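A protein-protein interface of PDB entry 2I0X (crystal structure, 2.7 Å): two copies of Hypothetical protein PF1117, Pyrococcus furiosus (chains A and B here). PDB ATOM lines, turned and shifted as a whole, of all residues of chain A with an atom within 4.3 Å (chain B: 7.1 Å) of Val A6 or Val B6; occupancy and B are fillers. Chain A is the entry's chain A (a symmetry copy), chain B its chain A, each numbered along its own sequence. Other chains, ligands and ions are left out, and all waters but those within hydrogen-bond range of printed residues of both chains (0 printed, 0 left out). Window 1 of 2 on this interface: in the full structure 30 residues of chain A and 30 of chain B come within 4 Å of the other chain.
N of Tyr B7 sits close to NE2 of Gln A29 (3.5 Å). The backbone NH (N) of Asp B8 lies close to the side-chain amide nitrogen (NE2) of Gln A29. The side-chain amide nitrogen (NE2) of Gln B29 lies close to the backbone NH (N) of Tyr A7, 3.5 Å away. OG of Ser B59 lies within hydrogen-bond range of OE1 of Gln A29 (3.0 Å).
Val B6 touches just these residues of chain A: Val A6 (3.7 Å), Gln A29 (3.7 Å) and Val A32 (3.3 Å). Printed residues of chain B within 4 Å of Ile A61: Gln B29. Printed residues of chain A within 4 Å of Asp B8: Gln A29. Of the printed residues of chain A, Gln B29 touches Val A6 (3.7 Å), Tyr A7 (3.1 Å) and Ile A61 (3.3 Å). Of the printed residues of chain A, Ile B61 touches Gln A29 (3.3 Å).
OH of Tyr B63 touches CG1 of Val A4, 3.8 Å away. Val B6 touches Val A6 (CG1 to CG1, 3.7 Å). O of Val A6 touches OE1 of Gln B29, at 3.7 Å. CG1 of Val A6 touches CG2 of Val B32, 3.3 Å away. O of Val B6 touches OE1 of Gln A29, 3.7 Å away. Gln A29 touches Ile B61 (OE1 to CG1, 3.3 Å). Val A32 touches Val B6. Val A32 touches Tyr B63. CG1 of Ile A61 touches OE1 of Gln B29 (3.3 Å).
The backbone NH of Tyr B63 is in hydrogen-bond range of the backbone carbonyl oxygen of Val B4 (3.1 Å). The backbone NH of Ile B61 sits at hydrogen-bond distance from the backbone carbonyl oxygen of Val B6 (2.9 Å). The backbone NH (N) of Tyr B7 sits at hydrogen-bond distance from the backbone carbonyl oxygen (O) of Ser B31. The backbone NH (N) of Asp B8 lies within hydrogen-bond range of the backbone carbonyl oxygen (O) of Ser B59, at 2.8 Å. O of Val A6 sits at hydrogen-bond distance from N of Ile A61 (2.9 Å). O of Ser A31 is in hydrogen-bond range of N of Tyr A7 (3.1 Å).
Printed residues of chain A that touch a printed residue of chain B: Val A4, Val A6, Tyr A7, Gln A29, Val A32 and Ile A61. Among the printed residues, no Asp or Glu carboxylate lies within 4 Å of a Lys or Arg side-chain nitrogen of the other chain.
Val A6 touches Gln B29, and with the chains exchanged Gln A29 touches Val B6. Val A6 touches Val B32, and with the chains exchanged Val A32 touches Val B6. Tyr A7 touches Gln B29, and with the chains exchanged Gln A29 touches Tyr B7. Gln A29 touches Ile B61, and with the chains exchanged Ile A61 touches Gln B29. Positions printed for both chains: 4, 5, 6, 7, 29, 31, 32, 60 and 61. Of the 13 pairs that touch across the chains among the printed residues, 9 have their exchanged pair printed and touching as well.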
ATOM      1  N   VAL A   4       6.169 -11.891 -24.879  1.00  0.00           N
ATOM      2  CA  VAL A   4       6.147 -12.857 -23.798  1.00  0.00           C
ATOM      3  C   VAL A   4       4.975 -12.386 -22.969  1.00  0.00           C
ATOM      4  O   VAL A   4       4.964 -11.259 -22.486  1.00  0.00           O
ATOM      5  CB  VAL A   4       7.427 -12.804 -22.924  1.00  0.00           C
ATOM      6  CG1 VAL A   4       8.635 -13.359 -23.679  1.00  0.00           C
ATOM      7  CG2 VAL A   4       7.695 -11.392 -22.527  1.00  0.00           C
ATOM      8  N   VAL A   5       3.971 -13.239 -22.830  1.00  0.00           N
ATOM      9  CA  VAL A   5       2.776 -12.913 -22.062  1.00  0.00           C
ATOM     10  C   VAL A   5       2.779 -13.655 -20.729  1.00  0.00           C
ATOM     11  O   VAL A   5       2.800 -14.886 -20.699  1.00  0.00           O
ATOM     12  CB  VAL A   5       1.515 -13.343 -22.826  1.00  0.00           C
ATOM     13  CG1 VAL A   5       0.269 -12.969 -22.036  1.00  0.00           C
ATOM     14  CG2 VAL A   5       1.500 -12.707 -24.196  1.00  0.00           C
ATOM     15  N   VAL A   6       2.758 -12.911 -19.630  1.00  0.00           N
ATOM     16  CA  VAL A   6       2.724 -13.530 -18.308  1.00  0.00           C
ATOM     17  C   VAL A   6       1.421 -13.070 -17.660  1.00  0.00           C
ATOM     18  O   VAL A   6       1.008 -11.924 -17.823  1.00  0.00           O
ATOM     19  CB  VAL A   6       3.914 -13.086 -17.433  1.00  0.00           C
ATOM     20  CG1 VAL A   6       3.989 -13.962 -16.182  1.00  0.00           C
ATOM     21  CG2 VAL A   6       5.195 -13.195 -18.210  1.00  0.00           C
ATOM     22  N   TYR A   7       0.756 -13.953 -16.932  1.00  0.00           N
ATOM     23  CA  TYR A   7      -0.501 -13.552 -16.325  1.00  0.00           C
ATOM     24  C   TYR A   7      -0.808 -14.170 -14.980  1.00  0.00           C
ATOM     25  O   TYR A   7      -0.338 -15.253 -14.629  1.00  0.00           O
ATOM     26  CB  TYR A   7      -1.656 -13.832 -17.290  1.00  0.00           C
ATOM     27  CG  TYR A   7      -1.769 -15.283 -17.690  1.00  0.00           C
ATOM     28  CD1 TYR A   7      -2.353 -16.221 -16.842  1.00  0.00           C
ATOM     29  CD2 TYR A   7      -1.278 -15.718 -18.915  1.00  0.00           C
ATOM     30  CE1 TYR A   7      -2.444 -17.551 -17.209  1.00  0.00           C
ATOM     31  CE2 TYR A   7      -1.364 -17.051 -19.290  1.00  0.00           C
ATOM     32  CZ  TYR A   7      -1.945 -17.964 -18.439  1.00  0.00           C
ATOM     33  OH  TYR A   7      -2.023 -19.289 -18.823  1.00  0.00           O
ATOM     34  N   GLN A  29       5.940 -22.002 -19.516  1.00  0.00           N
ATOM     35  CA  GLN A  29       5.749 -22.557 -18.191  1.00  0.00           C
ATOM     36  C   GLN A  29       4.368 -22.107 -17.801  1.00  0.00           C
ATOM     37  O   GLN A  29       3.687 -21.451 -18.589  1.00  0.00           O
ATOM     38  CB  GLN A  29       6.797 -22.069 -17.159  1.00  0.00           C
ATOM     39  CG  GLN A  29       6.683 -20.613 -16.710  1.00  0.00           C
ATOM     40  CD  GLN A  29       7.553 -20.267 -15.472  1.00  0.00           C
ATOM     41  OE1 GLN A  29       8.753 -20.583 -15.418  1.00  0.00           O
ATOM     42  NE2 GLN A  29       6.942 -19.590 -14.489  1.00  0.00           N
ATOM     43  N   SER A  31       1.513 -20.082 -16.691  1.00  0.00           N
ATOM     44  CA  SER A  31       1.242 -18.646 -16.703  1.00  0.00           C
ATOM     45  C   SER A  31       2.153 -17.865 -17.636  1.00  0.00           C
ATOM     46  O   SER A  31       2.138 -16.634 -17.639  1.00  0.00           O
ATOM     47  CB  SER A  31       1.331 -18.078 -15.287  1.00  0.00           C
ATOM     48  OG  SER A  31       0.266 -18.566 -14.491  1.00  0.00           O
ATOM     49  N   VAL A  32       2.931 -18.577 -18.441  1.00  0.00           N
ATOM     50  CA  VAL A  32       3.817 -17.910 -19.377  1.00  0.00           C
ATOM     51  C   VAL A  32       3.725 -18.445 -20.813  1.00  0.00           C
ATOM     52  O   VAL A  32       3.887 -19.630 -21.046  1.00  0.00           O
ATOM     53  CB  VAL A  32       5.296 -18.007 -18.905  1.00  0.00           C
ATOM     54  CG1 VAL A  32       6.191 -17.188 -19.826  1.00  0.00           C
ATOM     55  CG2 VAL A  32       5.420 -17.524 -17.474  1.00  0.00           C
ATOM     56  N   VAL A  60      -2.439  -9.021 -16.343  1.00  0.00           N
ATOM     57  CA  VAL A  60      -1.748  -9.590 -17.497  1.00  0.00           C
ATOM     58  C   VAL A  60      -0.685  -8.642 -18.026  1.00  0.00           C
ATOM     59  O   VAL A  60      -0.984  -7.494 -18.342  1.00  0.00           O
ATOM     60  CB  VAL A  60      -2.714  -9.918 -18.656  1.00  0.00           C
ATOM     61  CG1 VAL A  60      -1.933 -10.485 -19.831  1.00  0.00           C
ATOM     62  CG2 VAL A  60      -3.771 -10.925 -18.197  1.00  0.00           C
ATOM     63  N   ILE A  61       0.559  -9.120 -18.105  1.00  0.00           N
ATOM     64  CA  ILE A  61       1.667  -8.317 -18.629  1.00  0.00           C
ATOM     65  C   ILE A  61       2.100  -8.889 -19.966  1.00  0.00           C
ATOM     66  O   ILE A  61       2.313 -10.109 -20.114  1.00  0.00           O
ATOM     67  CB  ILE A  61       2.923  -8.314 -17.703  1.00  0.00           C
ATOM     68  CG1 ILE A  61       2.555  -7.792 -16.309  1.00  0.00           C
ATOM     69  CG2 ILE A  61       4.011  -7.409 -18.295  1.00  0.00           C
ATOM     70  CD1 ILE A  61       3.681  -7.844 -15.319  1.00  0.00           C
ATOM     71  N   VAL B   4      13.997 -10.298 -16.793  1.00  0.00           N
ATOM     72  CA  VAL B   4      12.641 -10.481 -16.313  1.00  0.00           C
ATOM     73  C   VAL B   4      12.660 -11.914 -15.837  1.00  0.00           C
ATOM     74  O   VAL B   4      12.927 -12.827 -16.610  1.00  0.00           O
ATOM     75  CB  VAL B   4      11.586 -10.347 -17.441  1.00  0.00           C
ATOM     76  CG1 VAL B   4      11.452  -8.895 -17.903  1.00  0.00           C
ATOM     77  CG2 VAL B   4      11.987 -11.201 -18.596  1.00  0.00           C
ATOM     78  N   VAL B   5      12.406 -12.110 -14.551  1.00  0.00           N
ATOM     79  CA  VAL B   5      12.397 -13.441 -13.955  1.00  0.00           C
ATOM     80  C   VAL B   5      10.967 -13.889 -13.672  1.00  0.00           C
ATOM     81  O   VAL B   5      10.247 -13.241 -12.911  1.00  0.00           O
ATOM     82  CB  VAL B   5      13.151 -13.434 -12.618  1.00  0.00           C
ATOM     83  CG1 VAL B   5      13.169 -14.832 -12.017  1.00  0.00           C
ATOM     84  CG2 VAL B   5      14.555 -12.912 -12.820  1.00  0.00           C
ATOM     85  N   VAL B   6      10.554 -14.994 -14.281  1.00  0.00           N
ATOM     86  CA  VAL B   6       9.214 -15.523 -14.046  1.00  0.00           C
ATOM     87  C   VAL B   6       9.406 -16.909 -13.436  1.00  0.00           C
ATOM     88  O   VAL B   6      10.308 -17.648 -13.827  1.00  0.00           O
ATOM     89  CB  VAL B   6       8.406 -15.648 -15.353  1.00  0.00           C
ATOM     90  CG1 VAL B   6       6.940 -15.932 -15.028  1.00  0.00           C
ATOM     91  CG2 VAL B   6       8.515 -14.379 -16.151  1.00  0.00           C
ATOM     92  N   TYR B   7       8.577 -17.273 -12.472  1.00  0.00           N
ATOM     93  CA  TYR B   7       8.753 -18.576 -11.855  1.00  0.00           C
ATOM     94  C   TYR B   7       7.485 -19.272 -11.416  1.00  0.00           C
ATOM     95  O   TYR B   7       6.456 -18.654 -11.135  1.00  0.00           O
ATOM     96  CB  TYR B   7       9.709 -18.461 -10.665  1.00  0.00           C
ATOM     97  CG  TYR B   7       9.238 -17.498  -9.603  1.00  0.00           C
ATOM     98  CD1 TYR B   7       8.259 -17.864  -8.680  1.00  0.00           C
ATOM     99  CD2 TYR B   7       9.765 -16.214  -9.531  1.00  0.00           C
ATOM    100  CE1 TYR B   7       7.824 -16.973  -7.718  1.00  0.00           C
ATOM    101  CE2 TYR B   7       9.331 -15.314  -8.567  1.00  0.00           C
ATOM    102  CZ  TYR B   7       8.364 -15.693  -7.664  1.00  0.00           C
ATOM    103  OH  TYR B   7       7.939 -14.788  -6.710  1.00  0.00           O
ATOM    104  N   ASP B   8       7.595 -20.589 -11.361  1.00  0.00           N
ATOM    105  CA  ASP B   8       6.508 -21.460 -10.956  1.00  0.00           C
ATOM    106  C   ASP B   8       7.093 -22.319  -9.845  1.00  0.00           C
ATOM    107  O   ASP B   8       7.743 -23.323 -10.118  1.00  0.00           O
ATOM    108  CB  ASP B   8       6.077 -22.312 -12.158  1.00  0.00           C
ATOM    109  CG  ASP B   8       5.022 -23.336 -11.804  1.00  0.00           C
ATOM    110  OD1 ASP B   8       4.171 -23.045 -10.923  1.00  0.00           O
ATOM    111  OD2 ASP B   8       5.038 -24.423 -12.429  1.00  0.00           O
ATOM    112  N   LEU B  21      14.136 -12.406  -4.310  1.00  0.00           N
ATOM    113  CA  LEU B  21      14.117 -11.517  -5.465  1.00  0.00           C
ATOM    114  C   LEU B  21      13.723 -10.092  -5.103  1.00  0.00           C
ATOM    115  O   LEU B  21      14.088  -9.152  -5.805  1.00  0.00           O
ATOM    116  CB  LEU B  21      13.154 -12.055  -6.521  1.00  0.00           C
ATOM    117  CG  LEU B  21      13.595 -13.379  -7.138  1.00  0.00           C
ATOM    118  CD1 LEU B  21      12.484 -14.005  -7.962  1.00  0.00           C
ATOM    119  CD2 LEU B  21      14.830 -13.118  -7.969  1.00  0.00           C
ATOM    120  N   GLN B  29       4.330  -8.442 -10.949  1.00  0.00           N
ATOM    121  CA  GLN B  29       3.075  -9.093 -10.635  1.00  0.00           C
ATOM    122  C   GLN B  29       3.484 -10.355  -9.925  1.00  0.00           C
ATOM    123  O   GLN B  29       4.674 -10.586  -9.713  1.00  0.00           O
ATOM    124  CB  GLN B  29       2.219  -9.422 -11.885  1.00  0.00           C
ATOM    125  CG  GLN B  29       2.730 -10.546 -12.784  1.00  0.00           C
ATOM    126  CD  GLN B  29       1.697 -11.028 -13.837  1.00  0.00           C
ATOM    127  OE1 GLN B  29       1.085 -10.222 -14.557  1.00  0.00           O
ATOM    128  NE2 GLN B  29       1.530 -12.355 -13.939  1.00  0.00           N
ATOM    129  N   ASN B  30       2.497 -11.147  -9.534  1.00  0.00           N
ATOM    130  CA  ASN B  30       2.748 -12.384  -8.834  1.00  0.00           C
ATOM    131  C   ASN B  30       3.567 -13.313  -9.719  1.00  0.00           C
ATOM    132  O   ASN B  30       3.176 -13.627 -10.858  1.00  0.00           O
ATOM    133  CB  ASN B  30       1.422 -13.041  -8.461  1.00  0.00           C
ATOM    134  CG  ASN B  30       1.594 -14.203  -7.491  1.00  0.00           C
ATOM    135  OD1 ASN B  30       1.951 -15.321  -7.884  1.00  0.00           O
ATOM    136  ND2 ASN B  30       1.350 -13.937  -6.207  1.00  0.00           N
ATOM    137  N   SER B  31       4.712 -13.737  -9.192  1.00  0.00           N
ATOM    138  CA  SER B  31       5.615 -14.646  -9.895  1.00  0.00           C
ATOM    139  C   SER B  31       6.462 -13.960 -10.954  1.00  0.00           C
ATOM    140  O   SER B  31       7.158 -14.622 -11.723  1.00  0.00           O
ATOM    141  CB  SER B  31       4.826 -15.797 -10.520  1.00  0.00           C
ATOM    142  OG  SER B  31       4.297 -16.639  -9.512  1.00  0.00           O
ATOM    143  N   VAL B  32       6.420 -12.634 -10.982  1.00  0.00           N
ATOM    144  CA  VAL B  32       7.215 -11.899 -11.950  1.00  0.00           C
ATOM    145  C   VAL B  32       8.037 -10.755 -11.341  1.00  0.00           C
ATOM    146  O   VAL B  32       7.497  -9.885 -10.680  1.00  0.00           O
ATOM    147  CB  VAL B  32       6.315 -11.318 -13.078  1.00  0.00           C
ATOM    148  CG1 VAL B  32       7.180 -10.669 -14.151  1.00  0.00           C
ATOM    149  CG2 VAL B  32       5.456 -12.414 -13.678  1.00  0.00           C
ATOM    150  N   PHE B  33       9.346 -10.776 -11.566  1.00  0.00           N
ATOM    151  CA  PHE B  33      10.235  -9.711 -11.100  1.00  0.00           C
ATOM    152  C   PHE B  33      11.130  -9.306 -12.277  1.00  0.00           C
ATOM    153  O   PHE B  33      11.451 -10.131 -13.136  1.00  0.00           O
ATOM    154  CB  PHE B  33      11.165 -10.172  -9.980  1.00  0.00           C
ATOM    155  CG  PHE B  33      10.498 -10.400  -8.658  1.00  0.00           C
ATOM    156  CD1 PHE B  33       9.737 -11.549  -8.433  1.00  0.00           C
ATOM    157  CD2 PHE B  33      10.740  -9.532  -7.593  1.00  0.00           C
ATOM    158  CE1 PHE B  33       9.245 -11.840  -7.171  1.00  0.00           C
ATOM    159  CE2 PHE B  33      10.247  -9.814  -6.318  1.00  0.00           C
ATOM    160  CZ  PHE B  33       9.500 -10.975  -6.105  1.00  0.00           C
ATOM    161  N   SER B  59      10.056 -24.571 -11.598  1.00  0.00           N
ATOM    162  CA  SER B  59      10.515 -24.004 -12.859  1.00  0.00           C
ATOM    163  C   SER B  59      10.776 -22.491 -12.776  1.00  0.00           C
ATOM    164  O   SER B  59       9.937 -21.724 -12.287  1.00  0.00           O
ATOM    165  CB  SER B  59       9.487 -24.271 -13.959  1.00  0.00           C
ATOM    166  OG  SER B  59       9.711 -23.402 -15.070  1.00  0.00           O
ATOM    167  N   VAL B  60      11.942 -22.064 -13.252  1.00  0.00           N
ATOM    168  CA  VAL B  60      12.273 -20.641 -13.257  1.00  0.00           C
ATOM    169  C   VAL B  60      12.857 -20.215 -14.593  1.00  0.00           C
ATOM    170  O   VAL B  60      13.839 -20.793 -15.050  1.00  0.00           O
ATOM    171  CB  VAL B  60      13.288 -20.273 -12.154  1.00  0.00           C
ATOM    172  CG1 VAL B  60      13.607 -18.788 -12.225  1.00  0.00           C
ATOM    173  CG2 VAL B  60      12.723 -20.619 -10.775  1.00  0.00           C
ATOM    174  N   ILE B  61      12.242 -19.213 -15.225  1.00  0.00           N
ATOM    175  CA  ILE B  61      12.725 -18.688 -16.505  1.00  0.00           C
ATOM    176  C   ILE B  61      13.279 -17.293 -16.285  1.00  0.00           C
ATOM    177  O   ILE B  61      12.638 -16.430 -15.653  1.00  0.00           O
ATOM    178  CB  ILE B  61      11.610 -18.574 -17.589  1.00  0.00           C
ATOM    179  CG1 ILE B  61      10.963 -19.942 -17.835  1.00  0.00           C
ATOM    180  CG2 ILE B  61      12.210 -18.071 -18.909  1.00  0.00           C
ATOM    181  CD1 ILE B  61       9.811 -19.912 -18.795  1.00  0.00           C
ATOM    182  N   ILE B  62      14.479 -17.074 -16.809  1.00  0.00           N
ATOM    183  CA  ILE B  62      15.135 -15.772 -16.702  1.00  0.00           C
ATOM    184  C   ILE B  62      15.537 -15.225 -18.065  1.00  0.00           C
ATOM    185  O   ILE B  62      16.596 -15.563 -18.594  1.00  0.00           O
ATOM    186  CB  ILE B  62      16.384 -15.834 -15.819  1.00  0.00           C
ATOM    187  CG1 ILE B  62      15.989 -16.282 -14.398  1.00  0.00           C
ATOM    188  CG2 ILE B  62      17.046 -14.457 -15.784  1.00  0.00           C
ATOM    189  CD1 ILE B  62      17.165 -16.501 -13.447  1.00  0.00           C
ATOM    190  N   TYR B  63      14.678 -14.382 -18.628  1.00  0.00           N
ATOM    191  CA  TYR B  63      14.955 -13.763 -19.913  1.00  0.00           C
ATOM    192  C   TYR B  63      16.060 -12.737 -19.756  1.00  0.00           C
ATOM    193  O   TYR B  63      16.053 -11.955 -18.809  1.00  0.00           O
ATOM    194  CB  TYR B  63      13.718 -13.067 -20.442  1.00  0.00           C
ATOM    195  CG  TYR B  63      12.579 -14.010 -20.696  1.00  0.00           C
ATOM    196  CD1 TYR B  63      11.565 -14.193 -19.744  1.00  0.00           C
ATOM    197  CD2 TYR B  63      12.488 -14.693 -21.906  1.00  0.00           C
ATOM    198  CE1 TYR B  63      10.485 -15.022 -20.005  1.00  0.00           C
ATOM    199  CE2 TYR B  63      11.414 -15.525 -22.173  1.00  0.00           C
ATOM    200  CZ  TYR B  63      10.418 -15.678 -21.231  1.00  0.00           C
ATOM    201  OH  TYR B  63       9.323 -16.427 -21.549  1.00  0.00           O
